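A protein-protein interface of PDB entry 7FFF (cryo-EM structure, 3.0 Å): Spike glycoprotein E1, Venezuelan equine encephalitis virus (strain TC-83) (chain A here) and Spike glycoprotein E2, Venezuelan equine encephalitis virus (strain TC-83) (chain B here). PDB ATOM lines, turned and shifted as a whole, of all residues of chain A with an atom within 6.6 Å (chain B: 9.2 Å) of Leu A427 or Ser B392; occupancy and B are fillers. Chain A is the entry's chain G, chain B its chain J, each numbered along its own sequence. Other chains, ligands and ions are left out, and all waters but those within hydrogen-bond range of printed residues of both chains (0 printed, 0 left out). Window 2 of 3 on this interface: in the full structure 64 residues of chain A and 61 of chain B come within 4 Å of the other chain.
Ser B392 touches three residues of chain A.
Gly A424 touches just one residue of chain B: Leu B388 (3.8 Å).
No residue of chain B comes within 4 Å of Val A426.
Of the printed residues of chain B, Ala A428 touches Ser B392.
No residue of chain B comes within 4 Å of Ile A430.
Of the printed residues of chain B, Leu A425 touches Leu B388 (3.9 Å).
Of the printed residues of chain A, Leu B388 touches Gly A424 (3.8 Å) and Leu A425 (3.9 Å).
Among the printed residues, merely in contact across the chains: Gly A424 with Leu B388 (3.8 Å), Leu A425 with Leu B388 (3.9 Å), Leu A427 with Ser B392 (3.7 Å), Ala A428 with Ser B392 (3.7 Å), Val A431 with Ser B392 (3.7 Å), Val A431 with Ala B395 (3.8 Å) and Val A431 with Cys B396 (3.7 Å).
Of the 18 printed residues of chain B, 4 touch a printed residue of chain A.
Printed residues of chain B that touch a printed residue of chain A: Leu B388, Ser B392, Ala B395 and Cys B396.
Of the 11 printed residues of chain A, 5 touch a printed residue of chain B.
Among the printed residues, 7 pairs touch across the chains.
The side-chain sulfur (SG) of Cys B396 is in hydrogen-bond range of the backbone carbonyl oxygen (O) of Ser B392.
The side-chain hydroxyl of Thr A429 is in hydrogen-bond range of the backbone carbonyl oxygen of Leu A425, 3.0 Å away.
The side-chain hydroxyl of Ser B392 lies within hydrogen-bond range of the backbone carbonyl oxygen of Leu B388 (2.9 Å).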
ATOM      1  N   ILE A 422       4.661 -15.502  11.785  1.00  0.00           N
ATOM      2  CA  ILE A 422       3.421 -16.217  12.073  1.00  0.00           C
ATOM      3  C   ILE A 422       3.157 -17.302  11.030  1.00  0.00           C
ATOM      4  O   ILE A 422       2.583 -18.347  11.366  1.00  0.00           O
ATOM      5  CB  ILE A 422       2.211 -15.275  12.222  1.00  0.00           C
ATOM      6  CG1 ILE A 422       1.890 -14.532  10.924  1.00  0.00           C
ATOM      7  CG2 ILE A 422       2.423 -14.314  13.383  1.00  0.00           C
ATOM      8  CD1 ILE A 422       0.569 -13.809  10.956  1.00  0.00           C
ATOM      9  N   ILE A 423       3.605 -17.127   9.779  1.00  0.00           N
ATOM     10  CA  ILE A 423       3.422 -18.234   8.843  1.00  0.00           C
ATOM     11  C   ILE A 423       4.421 -19.344   9.138  1.00  0.00           C
ATOM     12  O   ILE A 423       4.127 -20.521   8.900  1.00  0.00           O
ATOM     13  CB  ILE A 423       3.484 -17.778   7.369  1.00  0.00           C
ATOM     14  CG1 ILE A 423       4.860 -17.239   6.982  1.00  0.00           C
ATOM     15  CG2 ILE A 423       2.391 -16.759   7.084  1.00  0.00           C
ATOM     16  CD1 ILE A 423       5.021 -16.995   5.502  1.00  0.00           C
ATOM     17  N   GLY A 424       5.573 -19.011   9.732  1.00  0.00           N
ATOM     18  CA  GLY A 424       6.467 -20.052  10.215  1.00  0.00           C
ATOM     19  C   GLY A 424       5.880 -20.842  11.371  1.00  0.00           C
ATOM     20  O   GLY A 424       6.022 -22.068  11.429  1.00  0.00           O
ATOM     21  N   LEU A 425       5.181 -20.161  12.285  1.00  0.00           N
ATOM     22  CA  LEU A 425       4.571 -20.872  13.411  1.00  0.00           C
ATOM     23  C   LEU A 425       3.393 -21.736  12.958  1.00  0.00           C
ATOM     24  O   LEU A 425       3.215 -22.862  13.451  1.00  0.00           O
ATOM     25  CB  LEU A 425       4.135 -19.876  14.482  1.00  0.00           C
ATOM     26  CG  LEU A 425       3.660 -20.479  15.806  1.00  0.00           C
ATOM     27  CD1 LEU A 425       4.796 -21.237  16.469  1.00  0.00           C
ATOM     28  CD2 LEU A 425       3.121 -19.407  16.737  1.00  0.00           C
ATOM     29  N   VAL A 426       2.593 -21.235  12.007  1.00  0.00           N
ATOM     30  CA  VAL A 426       1.496 -22.032  11.451  1.00  0.00           C
ATOM     31  C   VAL A 426       2.034 -23.241  10.689  1.00  0.00           C
ATOM     32  O   VAL A 426       1.486 -24.350  10.795  1.00  0.00           O
ATOM     33  CB  VAL A 426       0.594 -21.139  10.573  1.00  0.00           C
ATOM     34  CG1 VAL A 426      -0.409 -21.961   9.780  1.00  0.00           C
ATOM     35  CG2 VAL A 426      -0.155 -20.152  11.446  1.00  0.00           C
ATOM     36  N   LEU A 427       3.141 -23.062   9.954  1.00  0.00           N
ATOM     37  CA  LEU A 427       3.758 -24.178   9.244  1.00  0.00           C
ATOM     38  C   LEU A 427       4.308 -25.215  10.217  1.00  0.00           C
ATOM     39  O   LEU A 427       4.205 -26.421   9.962  1.00  0.00           O
ATOM     40  CB  LEU A 427       4.853 -23.646   8.316  1.00  0.00           C
ATOM     41  CG  LEU A 427       5.460 -24.438   7.144  1.00  0.00           C
ATOM     42  CD1 LEU A 427       6.516 -25.452   7.558  1.00  0.00           C
ATOM     43  CD2 LEU A 427       4.358 -25.106   6.333  1.00  0.00           C
ATOM     44  N   ALA A 428       4.859 -24.765  11.352  1.00  0.00           N
ATOM     45  CA  ALA A 428       5.334 -25.695  12.376  1.00  0.00           C
ATOM     46  C   ALA A 428       4.187 -26.497  12.980  1.00  0.00           C
ATOM     47  O   ALA A 428       4.319 -27.709  13.212  1.00  0.00           O
ATOM     48  CB  ALA A 428       6.084 -24.934  13.467  1.00  0.00           C
ATOM     49  N   THR A 429       3.044 -25.842  13.218  1.00  0.00           N
ATOM     50  CA  THR A 429       1.885 -26.546  13.771  1.00  0.00           C
ATOM     51  C   THR A 429       1.324 -27.568  12.783  1.00  0.00           C
ATOM     52  O   THR A 429       0.985 -28.696  13.171  1.00  0.00           O
ATOM     53  CB  THR A 429       0.813 -25.533  14.178  1.00  0.00           C
ATOM     54  OG1 THR A 429       1.371 -24.606  15.119  1.00  0.00           O
ATOM     55  CG2 THR A 429      -0.376 -26.231  14.826  1.00  0.00           C
ATOM     56  N   ILE A 430       1.262 -27.205  11.498  1.00  0.00           N
ATOM     57  CA  ILE A 430       0.768 -28.124  10.472  1.00  0.00           C
ATOM     58  C   ILE A 430       1.714 -29.313  10.301  1.00  0.00           C
ATOM     59  O   ILE A 430       1.266 -30.457  10.149  1.00  0.00           O
ATOM     60  CB  ILE A 430       0.536 -27.361   9.151  1.00  0.00           C
ATOM     61  CG1 ILE A 430      -0.641 -26.394   9.299  1.00  0.00           C
ATOM     62  CG2 ILE A 430       0.294 -28.297   7.975  1.00  0.00           C
ATOM     63  CD1 ILE A 430      -0.823 -25.481   8.119  1.00  0.00           C
ATOM     64  N   VAL A 431       3.028 -29.076  10.384  1.00  0.00           N
ATOM     65  CA  VAL A 431       3.999 -30.167  10.293  1.00  0.00           C
ATOM     66  C   VAL A 431       3.886 -31.107  11.492  1.00  0.00           C
ATOM     67  O   VAL A 431       3.960 -32.334  11.336  1.00  0.00           O
ATOM     68  CB  VAL A 431       5.418 -29.588  10.123  1.00  0.00           C
ATOM     69  CG1 VAL A 431       6.492 -30.619  10.405  1.00  0.00           C
ATOM     70  CG2 VAL A 431       5.593 -29.093   8.699  1.00  0.00           C
ATOM     71  N   ALA A 432       3.648 -30.560  12.691  1.00  0.00           N
ATOM     72  CA  ALA A 432       3.455 -31.408  13.869  1.00  0.00           C
ATOM     73  C   ALA A 432       2.193 -32.261  13.758  1.00  0.00           C
ATOM     74  O   ALA A 432       2.209 -33.458  14.095  1.00  0.00           O
ATOM     75  CB  ALA A 432       3.409 -30.550  15.130  1.00  0.00           C
ATOM     76  N   ALA B 384      14.452 -16.811  13.526  1.00  0.00           N
ATOM     77  CA  ALA B 384      13.523 -17.773  14.108  1.00  0.00           C
ATOM     78  C   ALA B 384      12.653 -18.436  13.044  1.00  0.00           C
ATOM     79  O   ALA B 384      12.293 -19.611  13.187  1.00  0.00           O
ATOM     80  CB  ALA B 384      12.656 -17.097  15.168  1.00  0.00           C
ATOM     81  N   SER B 385      12.344 -17.724  11.956  1.00  0.00           N
ATOM     82  CA  SER B 385      11.587 -18.339  10.872  1.00  0.00           C
ATOM     83  C   SER B 385      12.409 -19.394  10.140  1.00  0.00           C
ATOM     84  O   SER B 385      11.884 -20.454   9.779  1.00  0.00           O
ATOM     85  CB  SER B 385      11.110 -17.274   9.894  1.00  0.00           C
ATOM     86  OG  SER B 385      10.424 -17.873   8.810  1.00  0.00           O
ATOM     87  N   THR B 386      13.700 -19.129   9.928  1.00  0.00           N
ATOM     88  CA  THR B 386      14.563 -20.132   9.311  1.00  0.00           C
ATOM     89  C   THR B 386      14.781 -21.320  10.243  1.00  0.00           C
ATOM     90  O   THR B 386      14.851 -22.466   9.778  1.00  0.00           O
ATOM     91  CB  THR B 386      15.891 -19.486   8.914  1.00  0.00           C
ATOM     92  OG1 THR B 386      15.628 -18.352   8.080  1.00  0.00           O
ATOM     93  CG2 THR B 386      16.768 -20.454   8.133  1.00  0.00           C
ATOM     94  N   TRP B 387      14.836 -21.066  11.557  1.00  0.00           N
ATOM     95  CA  TRP B 387      14.927 -22.136  12.548  1.00  0.00           C
ATOM     96  C   TRP B 387      13.705 -23.049  12.495  1.00  0.00           C
ATOM     97  O   TRP B 387      13.834 -24.282  12.461  1.00  0.00           O
ATOM     98  CB  TRP B 387      15.080 -21.519  13.937  1.00  0.00           C
ATOM     99  CG  TRP B 387      15.247 -22.489  15.062  1.00  0.00           C
ATOM    100  CD1 TRP B 387      16.293 -23.342  15.263  1.00  0.00           C
ATOM    101  CD2 TRP B 387      14.356 -22.681  16.163  1.00  0.00           C
ATOM    102  NE1 TRP B 387      16.102 -24.062  16.416  1.00  0.00           N
ATOM    103  CE2 TRP B 387      14.919 -23.676  16.989  1.00  0.00           C
ATOM    104  CE3 TRP B 387      13.131 -22.113  16.530  1.00  0.00           C
ATOM    105  CZ2 TRP B 387      14.299 -24.115  18.158  1.00  0.00           C
ATOM    106  CZ3 TRP B 387      12.518 -22.550  17.690  1.00  0.00           C
ATOM    107  CH2 TRP B 387      13.101 -23.541  18.490  1.00  0.00           C
ATOM    108  N   LEU B 388      12.509 -22.452  12.457  1.00  0.00           N
ATOM    109  CA  LEU B 388      11.285 -23.243  12.357  1.00  0.00           C
ATOM    110  C   LEU B 388      11.177 -23.971  11.024  1.00  0.00           C
ATOM    111  O   LEU B 388      10.686 -25.103  10.987  1.00  0.00           O
ATOM    112  CB  LEU B 388      10.059 -22.358  12.571  1.00  0.00           C
ATOM    113  CG  LEU B 388       9.842 -21.815  13.983  1.00  0.00           C
ATOM    114  CD1 LEU B 388       8.646 -20.880  14.012  1.00  0.00           C
ATOM    115  CD2 LEU B 388       9.660 -22.954  14.968  1.00  0.00           C
ATOM    116  N   PHE B 389      11.648 -23.358   9.931  1.00  0.00           N
ATOM    117  CA  PHE B 389      11.598 -24.025   8.633  1.00  0.00           C
ATOM    118  C   PHE B 389      12.534 -25.225   8.582  1.00  0.00           C
ATOM    119  O   PHE B 389      12.174 -26.275   8.036  1.00  0.00           O
ATOM    120  CB  PHE B 389      11.942 -23.043   7.515  1.00  0.00           C
ATOM    121  CG  PHE B 389      11.891 -23.648   6.141  1.00  0.00           C
ATOM    122  CD1 PHE B 389      10.673 -23.896   5.527  1.00  0.00           C
ATOM    123  CD2 PHE B 389      13.059 -23.967   5.461  1.00  0.00           C
ATOM    124  CE1 PHE B 389      10.618 -24.452   4.259  1.00  0.00           C
ATOM    125  CE2 PHE B 389      13.012 -24.527   4.196  1.00  0.00           C
ATOM    126  CZ  PHE B 389      11.789 -24.767   3.594  1.00  0.00           C
ATOM    127  N   CYS B 390      13.734 -25.096   9.157  1.00  0.00           N
ATOM    128  CA  CYS B 390      14.665 -26.222   9.176  1.00  0.00           C
ATOM    129  C   CYS B 390      14.162 -27.345  10.075  1.00  0.00           C
ATOM    130  O   CYS B 390      14.285 -28.525   9.721  1.00  0.00           O
ATOM    131  CB  CYS B 390      16.051 -25.758   9.618  1.00  0.00           C
ATOM    132  SG  CYS B 390      16.898 -24.689   8.434  1.00  0.00           S
ATOM    133  N   ARG B 391      13.568 -27.000  11.223  1.00  0.00           N
ATOM    134  CA  ARG B 391      13.024 -28.049  12.083  1.00  0.00           C
ATOM    135  C   ARG B 391      11.799 -28.714  11.469  1.00  0.00           C
ATOM    136  O   ARG B 391      11.598 -29.918  11.652  1.00  0.00           O
ATOM    137  CB  ARG B 391      12.695 -27.496  13.464  1.00  0.00           C
ATOM    138  CG  ARG B 391      13.921 -27.105  14.250  1.00  0.00           C
ATOM    139  CD  ARG B 391      13.538 -26.597  15.620  1.00  0.00           C
ATOM    140  NE  ARG B 391      12.977 -27.649  16.459  1.00  0.00           N
ATOM    141  CZ  ARG B 391      13.705 -28.451  17.229  1.00  0.00           C
ATOM    142  NH1 ARG B 391      15.023 -28.321  17.262  1.00  0.00           N
ATOM    143  NH2 ARG B 391      13.113 -29.381  17.967  1.00  0.00           N
ATOM    144  N   SER B 392      11.002 -27.970  10.697  1.00  0.00           N
ATOM    145  CA  SER B 392       9.875 -28.584  10.005  1.00  0.00           C
ATOM    146  C   SER B 392      10.346 -29.487   8.871  1.00  0.00           C
ATOM    147  O   SER B 392       9.742 -30.536   8.620  1.00  0.00           O
ATOM    148  CB  SER B 392       8.933 -27.506   9.477  1.00  0.00           C
ATOM    149  OG  SER B 392       8.339 -26.786  10.541  1.00  0.00           O
ATOM    150  N   ARG B 393      11.431 -29.105   8.190  1.00  0.00           N
ATOM    151  CA  ARG B 393      11.976 -29.958   7.137  1.00  0.00           C
ATOM    152  C   ARG B 393      12.543 -31.251   7.711  1.00  0.00           C
ATOM    153  O   ARG B 393      12.333 -32.329   7.140  1.00  0.00           O
ATOM    154  CB  ARG B 393      13.051 -29.210   6.350  1.00  0.00           C
ATOM    155  CG  ARG B 393      13.589 -29.996   5.165  1.00  0.00           C
ATOM    156  CD  ARG B 393      14.654 -29.235   4.401  1.00  0.00           C
ATOM    157  NE  ARG B 393      15.110 -29.968   3.225  1.00  0.00           N
ATOM    158  CZ  ARG B 393      16.101 -30.852   3.234  1.00  0.00           C
ATOM    159  NH1 ARG B 393      16.743 -31.124   4.360  1.00  0.00           N
ATOM    160  NH2 ARG B 393      16.447 -31.472   2.114  1.00  0.00           N
ATOM    161  N   VAL B 394      13.237 -31.159   8.849  1.00  0.00           N
ATOM    162  CA  VAL B 394      13.741 -32.359   9.516  1.00  0.00           C
ATOM    163  C   VAL B 394      12.589 -33.226  10.015  1.00  0.00           C
ATOM    164  O   VAL B 394      12.618 -34.455   9.874  1.00  0.00           O
ATOM    165  CB  VAL B 394      14.706 -31.964  10.653  1.00  0.00           C
ATOM    166  CG1 VAL B 394      15.095 -33.163  11.499  1.00  0.00           C
ATOM    167  CG2 VAL B 394      15.957 -31.332  10.068  1.00  0.00           C
ATOM    168  N   ALA B 395      11.533 -32.602  10.547  1.00  0.00           N
ATOM    169  CA  ALA B 395      10.393 -33.361  11.050  1.00  0.00           C
ATOM    170  C   ALA B 395       9.608 -34.038   9.932  1.00  0.00           C
ATOM    171  O   ALA B 395       9.005 -35.093  10.154  1.00  0.00           O
ATOM    172  CB  ALA B 395       9.475 -32.446  11.859  1.00  0.00           C
ATOM    173  N   CYS B 396       9.598 -33.457   8.731  1.00  0.00           N
ATOM    174  CA  CYS B 396       8.930 -34.120   7.617  1.00  0.00           C
ATOM    175  C   CYS B 396       9.804 -35.168   6.943  1.00  0.00           C
ATOM    176  O   CYS B 396       9.277 -36.131   6.378  1.00  0.00           O
ATOM    177  CB  CYS B 396       8.476 -33.099   6.575  1.00  0.00           C
ATOM    178  SG  CYS B 396       7.130 -32.036   7.100  1.00  0.00           S
ATOM    179  N   LEU B 397      11.126 -35.006   6.968  1.00  0.00           N
ATOM    180  CA  LEU B 397      11.977 -35.933   6.238  1.00  0.00           C
ATOM    181  C   LEU B 397      12.624 -37.002   7.109  1.00  0.00           C
ATOM    182  O   LEU B 397      13.284 -37.888   6.567  1.00  0.00           O
ATOM    183  CB  LEU B 397      13.068 -35.166   5.488  1.00  0.00           C
ATOM    184  CG  LEU B 397      12.552 -34.266   4.366  1.00  0.00           C
ATOM    185  CD1 LEU B 397      13.688 -33.476   3.743  1.00  0.00           C
ATOM    186  CD2 LEU B 397      11.819 -35.082   3.312  1.00  0.00           C
ATOM    187  N   THR B 398      12.463 -36.952   8.432  1.00  0.00           N
ATOM    188  CA  THR B 398      13.113 -37.961   9.269  1.00  0.00           C
ATOM    189  C   THR B 398      12.457 -39.341   9.205  1.00  0.00           C
ATOM    190  O   THR B 398      13.189 -40.322   8.983  1.00  0.00           O
ATOM    191  CB  THR B 398      13.252 -37.430  10.705  1.00  0.00           C
ATOM    192  OG1 THR B 398      14.088 -36.268  10.700  1.00  0.00           O
ATOM    193  CG2 THR B 398      13.864 -38.472  11.619  1.00  0.00           C
ATOM    194  N   PRO B 399      11.126 -39.518   9.375  1.00  0.00           N
ATOM    195  CA  PRO B 399      10.604 -40.900   9.370  1.00  0.00           C
ATOM    196  C   PRO B 399      10.591 -41.552   7.997  1.00  0.00           C
ATOM    197  O   PRO B 399      10.538 -42.785   7.918  1.00  0.00           O
ATOM    198  CB  PRO B 399       9.176 -40.746   9.911  1.00  0.00           C
ATOM    199  CG  PRO B 399       9.141 -39.438  10.561  1.00  0.00           C
ATOM    200  CD  PRO B 399      10.022 -38.598   9.712  1.00  0.00           C
ATOM    201  N   LEU B 415       8.983 -30.782  -2.983  1.00  0.00           N
ATOM    202  CA  LEU B 415       8.758 -29.644  -2.092  1.00  0.00           C
ATOM    203  C   LEU B 415       9.899 -29.469  -1.096  1.00  0.00           C
ATOM    204  O   LEU B 415      10.563 -28.428  -1.070  1.00  0.00           O
ATOM    205  CB  LEU B 415       7.428 -29.804  -1.351  1.00  0.00           C
ATOM    206  CG  LEU B 415       6.143 -29.665  -2.166  1.00  0.00           C
ATOM    207  CD1 LEU B 415       4.925 -29.961  -1.301  1.00  0.00           C
ATOM    208  CD2 LEU B 415       6.050 -28.278  -2.776  1.00  0.00           C
ATOM    209  N   CYS B 416      10.154 -30.486  -0.275  1.00  0.00           N
ATOM    210  CA  CYS B 416      11.111 -30.362   0.817  1.00  0.00           C
ATOM    211  C   CYS B 416      12.556 -30.605   0.392  1.00  0.00           C
ATOM    212  O   CYS B 416      13.386 -30.886   1.264  1.00  0.00           O
ATOM    213  CB  CYS B 416      10.732 -31.309   1.955  1.00  0.00           C
ATOM    214  SG  CYS B 416       9.162 -30.900   2.743  1.00  0.00           S
